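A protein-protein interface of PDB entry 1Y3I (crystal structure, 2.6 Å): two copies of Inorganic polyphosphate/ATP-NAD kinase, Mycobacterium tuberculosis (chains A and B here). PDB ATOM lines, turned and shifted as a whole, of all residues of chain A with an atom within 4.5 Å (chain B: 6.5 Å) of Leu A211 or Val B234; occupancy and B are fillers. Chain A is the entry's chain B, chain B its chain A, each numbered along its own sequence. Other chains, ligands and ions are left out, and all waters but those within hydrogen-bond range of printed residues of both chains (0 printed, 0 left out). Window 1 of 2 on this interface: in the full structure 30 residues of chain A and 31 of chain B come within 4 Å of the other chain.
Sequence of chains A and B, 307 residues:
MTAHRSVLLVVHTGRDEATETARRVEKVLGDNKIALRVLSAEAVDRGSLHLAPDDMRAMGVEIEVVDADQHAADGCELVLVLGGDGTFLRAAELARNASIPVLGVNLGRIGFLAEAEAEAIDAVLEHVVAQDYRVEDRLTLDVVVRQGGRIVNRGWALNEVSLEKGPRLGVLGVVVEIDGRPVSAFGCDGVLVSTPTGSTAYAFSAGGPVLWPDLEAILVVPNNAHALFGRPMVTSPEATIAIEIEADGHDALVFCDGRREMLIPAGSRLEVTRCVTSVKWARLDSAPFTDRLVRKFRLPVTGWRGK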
ATOM      1  N   PRO A 196       2.228  14.327 -17.731  1.00  0.00           N
ATOM      2  CA  PRO A 196       2.357  15.130 -16.512  1.00  0.00           C
ATOM      3  C   PRO A 196       1.330  14.697 -15.475  1.00  0.00           C
ATOM      4  O   PRO A 196       1.565  14.648 -14.270  1.00  0.00           O
ATOM      5  CB  PRO A 196       2.027  16.543 -17.000  1.00  0.00           C
ATOM      6  CG  PRO A 196       2.522  16.529 -18.419  1.00  0.00           C
ATOM      7  CD  PRO A 196       2.129  15.169 -18.939  1.00  0.00           C
ATOM      8  N   SER A 199       2.874  12.101 -13.788  1.00  0.00           N
ATOM      9  CA  SER A 199       4.277  12.377 -13.521  1.00  0.00           C
ATOM     10  C   SER A 199       4.753  11.888 -12.157  1.00  0.00           C
ATOM     11  O   SER A 199       5.952  11.630 -12.000  1.00  0.00           O
ATOM     12  CB  SER A 199       4.535  13.882 -13.622  1.00  0.00           C
ATOM     13  OG  SER A 199       3.966  14.594 -12.542  1.00  0.00           O
ATOM     14  N   PRO A 209      10.905  13.696 -12.588  1.00  0.00           N
ATOM     15  CA  PRO A 209      10.549  14.946 -11.911  1.00  0.00           C
ATOM     16  C   PRO A 209       9.049  14.952 -11.675  1.00  0.00           C
ATOM     17  O   PRO A 209       8.288  14.224 -12.322  1.00  0.00           O
ATOM     18  CB  PRO A 209      10.909  16.018 -12.929  1.00  0.00           C
ATOM     19  CG  PRO A 209      10.767  15.346 -14.256  1.00  0.00           C
ATOM     20  CD  PRO A 209      10.992  13.874 -14.047  1.00  0.00           C
ATOM     21  N   VAL A 210       8.610  15.780 -10.735  1.00  0.00           N
ATOM     22  CA  VAL A 210       7.150  15.878 -10.595  1.00  0.00           C
ATOM     23  C   VAL A 210       6.621  16.840 -11.643  1.00  0.00           C
ATOM     24  O   VAL A 210       7.132  17.962 -11.717  1.00  0.00           O
ATOM     25  CB  VAL A 210       6.801  16.327  -9.170  1.00  0.00           C
ATOM     26  CG1 VAL A 210       5.305  16.505  -8.969  1.00  0.00           C
ATOM     27  CG2 VAL A 210       7.372  15.297  -8.204  1.00  0.00           C
ATOM     28  N   LEU A 211       5.641  16.442 -12.449  1.00  0.00           N
ATOM     29  CA  LEU A 211       5.014  17.421 -13.336  1.00  0.00           C
ATOM     30  C   LEU A 211       3.635  17.794 -12.776  1.00  0.00           C
ATOM     31  O   LEU A 211       2.904  16.884 -12.386  1.00  0.00           O
ATOM     32  CB  LEU A 211       4.846  16.952 -14.763  1.00  0.00           C
ATOM     33  CG  LEU A 211       6.057  16.367 -15.485  1.00  0.00           C
ATOM     34  CD1 LEU A 211       5.655  15.885 -16.869  1.00  0.00           C
ATOM     35  CD2 LEU A 211       7.174  17.390 -15.565  1.00  0.00           C
ATOM     36  N   TRP A 212       3.388  19.100 -12.769  1.00  0.00           N
ATOM     37  CA  TRP A 212       2.098  19.665 -12.363  1.00  0.00           C
ATOM     38  C   TRP A 212       1.091  19.338 -13.473  1.00  0.00           C
ATOM     39  O   TRP A 212       1.330  19.663 -14.641  1.00  0.00           O
ATOM     40  CB  TRP A 212       2.166  21.158 -12.120  1.00  0.00           C
ATOM     41  CG  TRP A 212       2.288  21.626 -10.708  1.00  0.00           C
ATOM     42  CD1 TRP A 212       1.499  22.542 -10.067  1.00  0.00           C
ATOM     43  CD2 TRP A 212       3.260  21.215  -9.740  1.00  0.00           C
ATOM     44  NE1 TRP A 212       1.912  22.727  -8.766  1.00  0.00           N
ATOM     45  CE2 TRP A 212       2.994  21.918  -8.546  1.00  0.00           C
ATOM     46  CE3 TRP A 212       4.327  20.313  -9.779  1.00  0.00           C
ATOM     47  CZ2 TRP A 212       3.755  21.755  -7.391  1.00  0.00           C
ATOM     48  CZ3 TRP A 212       5.078  20.154  -8.634  1.00  0.00           C
ATOM     49  CH2 TRP A 212       4.789  20.865  -7.468  1.00  0.00           C
ATOM     50  N   PRO A 213       0.006  18.690 -13.076  1.00  0.00           N
ATOM     51  CA  PRO A 213      -0.953  17.996 -13.928  1.00  0.00           C
ATOM     52  C   PRO A 213      -1.417  18.777 -15.158  1.00  0.00           C
ATOM     53  O   PRO A 213      -1.725  18.194 -16.208  1.00  0.00           O
ATOM     54  CB  PRO A 213      -2.166  17.792 -13.010  1.00  0.00           C
ATOM     55  CG  PRO A 213      -1.879  18.545 -11.762  1.00  0.00           C
ATOM     56  CD  PRO A 213      -0.379  18.596 -11.652  1.00  0.00           C
ATOM     57  N   LEU A 215       0.303  20.943 -16.933  1.00  0.00           N
ATOM     58  CA  LEU A 215       1.276  21.204 -17.988  1.00  0.00           C
ATOM     59  C   LEU A 215       0.805  20.602 -19.312  1.00  0.00           C
ATOM     60  O   LEU A 215      -0.110  19.777 -19.326  1.00  0.00           O
ATOM     61  CB  LEU A 215       2.643  20.598 -17.682  1.00  0.00           C
ATOM     62  CG  LEU A 215       3.679  21.563 -17.102  1.00  0.00           C
ATOM     63  CD1 LEU A 215       3.136  22.093 -15.789  1.00  0.00           C
ATOM     64  CD2 LEU A 215       5.009  20.868 -16.939  1.00  0.00           C
ATOM     65  N   LEU A 219       6.496  13.203 -20.906  1.00  0.00           N
ATOM     66  CA  LEU A 219       7.579  12.743 -20.045  1.00  0.00           C
ATOM     67  C   LEU A 219       8.237  11.467 -20.563  1.00  0.00           C
ATOM     68  O   LEU A 219       7.590  10.447 -20.804  1.00  0.00           O
ATOM     69  CB  LEU A 219       7.016  12.497 -18.652  1.00  0.00           C
ATOM     70  CG  LEU A 219       7.864  12.757 -17.419  1.00  0.00           C
ATOM     71  CD1 LEU A 219       7.484  11.760 -16.331  1.00  0.00           C
ATOM     72  CD2 LEU A 219       9.351  12.682 -17.716  1.00  0.00           C
ATOM     73  N   VAL A 234      11.783  16.030 -20.919  1.00  0.00           N
ATOM     74  CA  VAL A 234      10.392  16.455 -21.080  1.00  0.00           C
ATOM     75  C   VAL A 234      10.194  17.268 -22.361  1.00  0.00           C
ATOM     76  O   VAL A 234      10.635  18.414 -22.454  1.00  0.00           O
ATOM     77  CB  VAL A 234       9.866  17.294 -19.901  1.00  0.00           C
ATOM     78  CG1 VAL A 234       8.347  17.321 -20.002  1.00  0.00           C
ATOM     79  CG2 VAL A 234      10.329  16.748 -18.565  1.00  0.00           C
ATOM     80  N   PHE A 289      -1.917  21.955  -7.134  1.00  0.00           N
ATOM     81  CA  PHE A 289      -1.372  20.598  -7.032  1.00  0.00           C
ATOM     82  C   PHE A 289      -0.493  20.486  -5.791  1.00  0.00           C
ATOM     83  O   PHE A 289      -0.425  19.457  -5.122  1.00  0.00           O
ATOM     84  CB  PHE A 289      -0.585  20.239  -8.283  1.00  0.00           C
ATOM     85  CG  PHE A 289       0.199  18.941  -8.263  1.00  0.00           C
ATOM     86  CD1 PHE A 289      -0.448  17.731  -8.443  1.00  0.00           C
ATOM     87  CD2 PHE A 289       1.571  18.921  -8.079  1.00  0.00           C
ATOM     88  CE1 PHE A 289       0.251  16.540  -8.440  1.00  0.00           C
ATOM     89  CE2 PHE A 289       2.284  17.738  -8.070  1.00  0.00           C
ATOM     90  CZ  PHE A 289       1.620  16.538  -8.252  1.00  0.00           C
ATOM     91  N   PRO B 209      16.318  17.861 -14.951  1.00  0.00           N
ATOM     92  CA  PRO B 209      15.973  17.124 -16.162  1.00  0.00           C
ATOM     93  C   PRO B 209      16.018  18.011 -17.395  1.00  0.00           C
ATOM     94  O   PRO B 209      16.163  19.228 -17.296  1.00  0.00           O
ATOM     95  CB  PRO B 209      14.515  16.720 -15.910  1.00  0.00           C
ATOM     96  CG  PRO B 209      13.958  17.858 -15.121  1.00  0.00           C
ATOM     97  CD  PRO B 209      15.097  18.337 -14.263  1.00  0.00           C
ATOM     98  N   LEU B 211      14.154  19.876 -20.308  1.00  0.00           N
ATOM     99  CA  LEU B 211      12.852  20.321 -20.791  1.00  0.00           C
ATOM    100  C   LEU B 211      12.945  20.805 -22.238  1.00  0.00           C
ATOM    101  O   LEU B 211      13.911  21.494 -22.571  1.00  0.00           O
ATOM    102  CB  LEU B 211      12.268  21.469 -19.979  1.00  0.00           C
ATOM    103  CG  LEU B 211      11.877  21.215 -18.528  1.00  0.00           C
ATOM    104  CD1 LEU B 211      11.126  22.430 -17.989  1.00  0.00           C
ATOM    105  CD2 LEU B 211      11.029  19.965 -18.353  1.00  0.00           C
ATOM    106  N   LEU B 215       8.811  24.736 -24.462  1.00  0.00           N
ATOM    107  CA  LEU B 215       7.915  24.528 -23.344  1.00  0.00           C
ATOM    108  C   LEU B 215       7.397  25.851 -22.781  1.00  0.00           C
ATOM    109  O   LEU B 215       8.001  26.908 -22.933  1.00  0.00           O
ATOM    110  CB  LEU B 215       8.619  23.783 -22.210  1.00  0.00           C
ATOM    111  CG  LEU B 215       8.239  22.345 -21.901  1.00  0.00           C
ATOM    112  CD1 LEU B 215       7.310  21.762 -22.956  1.00  0.00           C
ATOM    113  CD2 LEU B 215       9.492  21.480 -21.761  1.00  0.00           C
ATOM    114  N   ALA B 217       6.389  26.358 -19.028  1.00  0.00           N
ATOM    115  CA  ALA B 217       6.471  25.691 -17.742  1.00  0.00           C
ATOM    116  C   ALA B 217       7.703  26.205 -17.010  1.00  0.00           C
ATOM    117  O   ALA B 217       8.606  26.750 -17.641  1.00  0.00           O
ATOM    118  CB  ALA B 217       6.552  24.185 -17.893  1.00  0.00           C
ATOM    119  N   ILE B 218       7.717  26.022 -15.699  1.00  0.00           N
ATOM    120  CA  ILE B 218       8.870  26.470 -14.909  1.00  0.00           C
ATOM    121  C   ILE B 218       9.506  25.325 -14.135  1.00  0.00           C
ATOM    122  O   ILE B 218       8.826  24.464 -13.564  1.00  0.00           O
ATOM    123  CB  ILE B 218       8.398  27.615 -13.997  1.00  0.00           C
ATOM    124  CG1 ILE B 218       7.888  28.811 -14.814  1.00  0.00           C
ATOM    125  CG2 ILE B 218       9.467  28.016 -13.006  1.00  0.00           C
ATOM    126  CD1 ILE B 218       6.926  29.674 -14.025  1.00  0.00           C
ATOM    127  N   LEU B 219      10.837  25.264 -14.117  1.00  0.00           N
ATOM    128  CA  LEU B 219      11.544  24.163 -13.474  1.00  0.00           C
ATOM    129  C   LEU B 219      12.187  24.589 -12.162  1.00  0.00           C
ATOM    130  O   LEU B 219      12.920  25.576 -12.071  1.00  0.00           O
ATOM    131  CB  LEU B 219      12.634  23.609 -14.388  1.00  0.00           C
ATOM    132  CG  LEU B 219      12.984  22.126 -14.344  1.00  0.00           C
ATOM    133  CD1 LEU B 219      14.497  21.944 -14.231  1.00  0.00           C
ATOM    134  CD2 LEU B 219      12.284  21.397 -13.211  1.00  0.00           C
ATOM    135  N   VAL B 220      11.922  23.810 -11.118  1.00  0.00           N
ATOM    136  CA  VAL B 220      12.571  24.083  -9.842  1.00  0.00           C
ATOM    137  C   VAL B 220      13.567  22.991  -9.481  1.00  0.00           C
ATOM    138  O   VAL B 220      13.241  21.823  -9.294  1.00  0.00           O
ATOM    139  CB  VAL B 220      11.534  24.230  -8.718  1.00  0.00           C
ATOM    140  CG1 VAL B 220      12.202  24.575  -7.394  1.00  0.00           C
ATOM    141  CG2 VAL B 220      10.520  25.290  -9.123  1.00  0.00           C
ATOM    142  N   PRO B 232      13.783  17.505  -8.735  1.00  0.00           N
ATOM    143  CA  PRO B 232      13.393  18.615  -9.608  1.00  0.00           C
ATOM    144  C   PRO B 232      11.874  18.653  -9.766  1.00  0.00           C
ATOM    145  O   PRO B 232      11.212  17.617  -9.851  1.00  0.00           O
ATOM    146  CB  PRO B 232      14.058  18.275 -10.937  1.00  0.00           C
ATOM    147  CG  PRO B 232      15.198  17.389 -10.571  1.00  0.00           C
ATOM    148  CD  PRO B 232      14.734  16.595  -9.381  1.00  0.00           C
ATOM    149  N   MET B 233      11.364  19.879  -9.795  1.00  0.00           N
ATOM    150  CA  MET B 233       9.946  20.154  -9.953  1.00  0.00           C
ATOM    151  C   MET B 233       9.685  20.933 -11.234  1.00  0.00           C
ATOM    152  O   MET B 233      10.214  22.025 -11.443  1.00  0.00           O
ATOM    153  CB  MET B 233       9.434  20.946  -8.751  1.00  0.00           C
ATOM    154  CG  MET B 233       9.091  20.098  -7.544  1.00  0.00           C
ATOM    155  SD  MET B 233       9.120  21.060  -6.008  1.00  0.00           S
ATOM    156  CE  MET B 233       8.371  19.876  -4.888  1.00  0.00           C
ATOM    157  N   VAL B 234       8.852  20.380 -12.110  1.00  0.00           N
ATOM    158  CA  VAL B 234       8.459  21.123 -13.308  1.00  0.00           C
ATOM    159  C   VAL B 234       7.061  21.708 -13.151  1.00  0.00           C
ATOM    160  O   VAL B 234       6.052  21.033 -13.360  1.00  0.00           O
ATOM    161  CB  VAL B 234       8.522  20.218 -14.544  1.00  0.00           C
ATOM    162  CG1 VAL B 234       8.190  20.981 -15.813  1.00  0.00           C
ATOM    163  CG2 VAL B 234       9.913  19.600 -14.643  1.00  0.00           C
ATOM    164  N   THR B 235       6.987  22.978 -12.772  1.00  0.00           N
ATOM    165  CA  THR B 235       5.730  23.639 -12.490  1.00  0.00           C
ATOM    166  C   THR B 235       5.044  24.213 -13.729  1.00  0.00           C
ATOM    167  O   THR B 235       5.624  24.375 -14.798  1.00  0.00           O
ATOM    168  CB  THR B 235       5.931  24.814 -11.510  1.00  0.00           C
ATOM    169  OG1 THR B 235       6.629  25.853 -12.219  1.00  0.00           O
ATOM    170  CG2 THR B 235       6.773  24.413 -10.316  1.00  0.00           C
ATOM    171  N   SER B 236       3.762  24.517 -13.527  1.00  0.00           N
ATOM    172  CA  SER B 236       2.951  25.144 -14.564  1.00  0.00           C
ATOM    173  C   SER B 236       3.257  26.631 -14.649  1.00  0.00           C
ATOM    174  O   SER B 236       3.310  27.308 -13.622  1.00  0.00           O
ATOM    175  CB  SER B 236       1.458  24.939 -14.309  1.00  0.00           C
ATOM    176  OG  SER B 236       1.222  24.791 -12.922  1.00  0.00           O
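N of Val B220 is in hydrogen-bond range of O of Met B233, at 2.5 Å.
The backbone carbonyl oxygen of Ile B218 is in hydrogen-bond range of the backbone NH of Thr B235, at 2.5 Å.
The side-chain hydroxyl (OG) of Ser A199 is in hydrogen-bond range of the backbone NH (N) of Leu A211, at 2.5 Å.
Ser A199 touches none of the printed residues of chain B.
Of chain B, only Val B234 (3.3 Å) comes within 4 Å of Leu A211.
Of the printed residues of chain B, Leu A215 touches Ala B217, Val B234, Thr B235 and Ser B236.
Printed residues of chain B within 4 Å of Val A234: Leu B211 (3.3 Å) and Leu B215 (3.3 Å).
Printed residues of chain A within 4 Å of Ala B217: Leu A215.
Ile B218 touches none of the printed residues of chain A.
Val B234 touches four residues of chain A.
The nearest printed residue of chain A that does not touch Pro B232 is Leu A211 (6.3 Å).
O of Val B234 lies within hydrogen-bond range of N of Trp A212, 3.3 Å away.
N of Val A210 is in hydrogen-bond range of O of Pro B232.
O of Val A210 sits at hydrogen-bond distance from N of Val B234 (3.0 Å).
Hydrophobic or aromatic side chains of chain A within 4 Å of the printed part of chain B: Pro A209, Leu A211, Trp A212, Leu A215 and Val A234.
Among the printed residues, 13 pairs touch across the chains.
Among the printed residues, no Asp or Glu carboxylate lies within 4 Å of a Lys or Arg side-chain nitrogen of the other chain.
Pro B232 touches Pro A209.
Met B233 touches Val A210.
CD2 of Leu A211 touches CB of Val B234, 3.3 Å away.
OG of Ser B236 touches CD1 of Trp A212, at 3.6 Å.
Leu A215 touches Ala B217.
Leu A215 touches Val B234.
CD1 of Leu A215 touches C of Thr B235, at 3.5 Å.
Leu A215 touches Ser B236.
Leu B211 touches Val A234.
Leu B215 touches Val A234 (CD2 to O, 3.3 Å).
Leu A211 touches Val B234, and with the chains exchanged Val A234 touches Leu B211.
Leu A215 touches Val B234, and with the chains exchanged Val A234 touches Leu B215.
Positions printed for both chains: 209, 211, 215, 219 and 234.
Of the 13 pairs that touch across the chains among the printed residues, 4 have their exchanged pair printed and touching as well.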
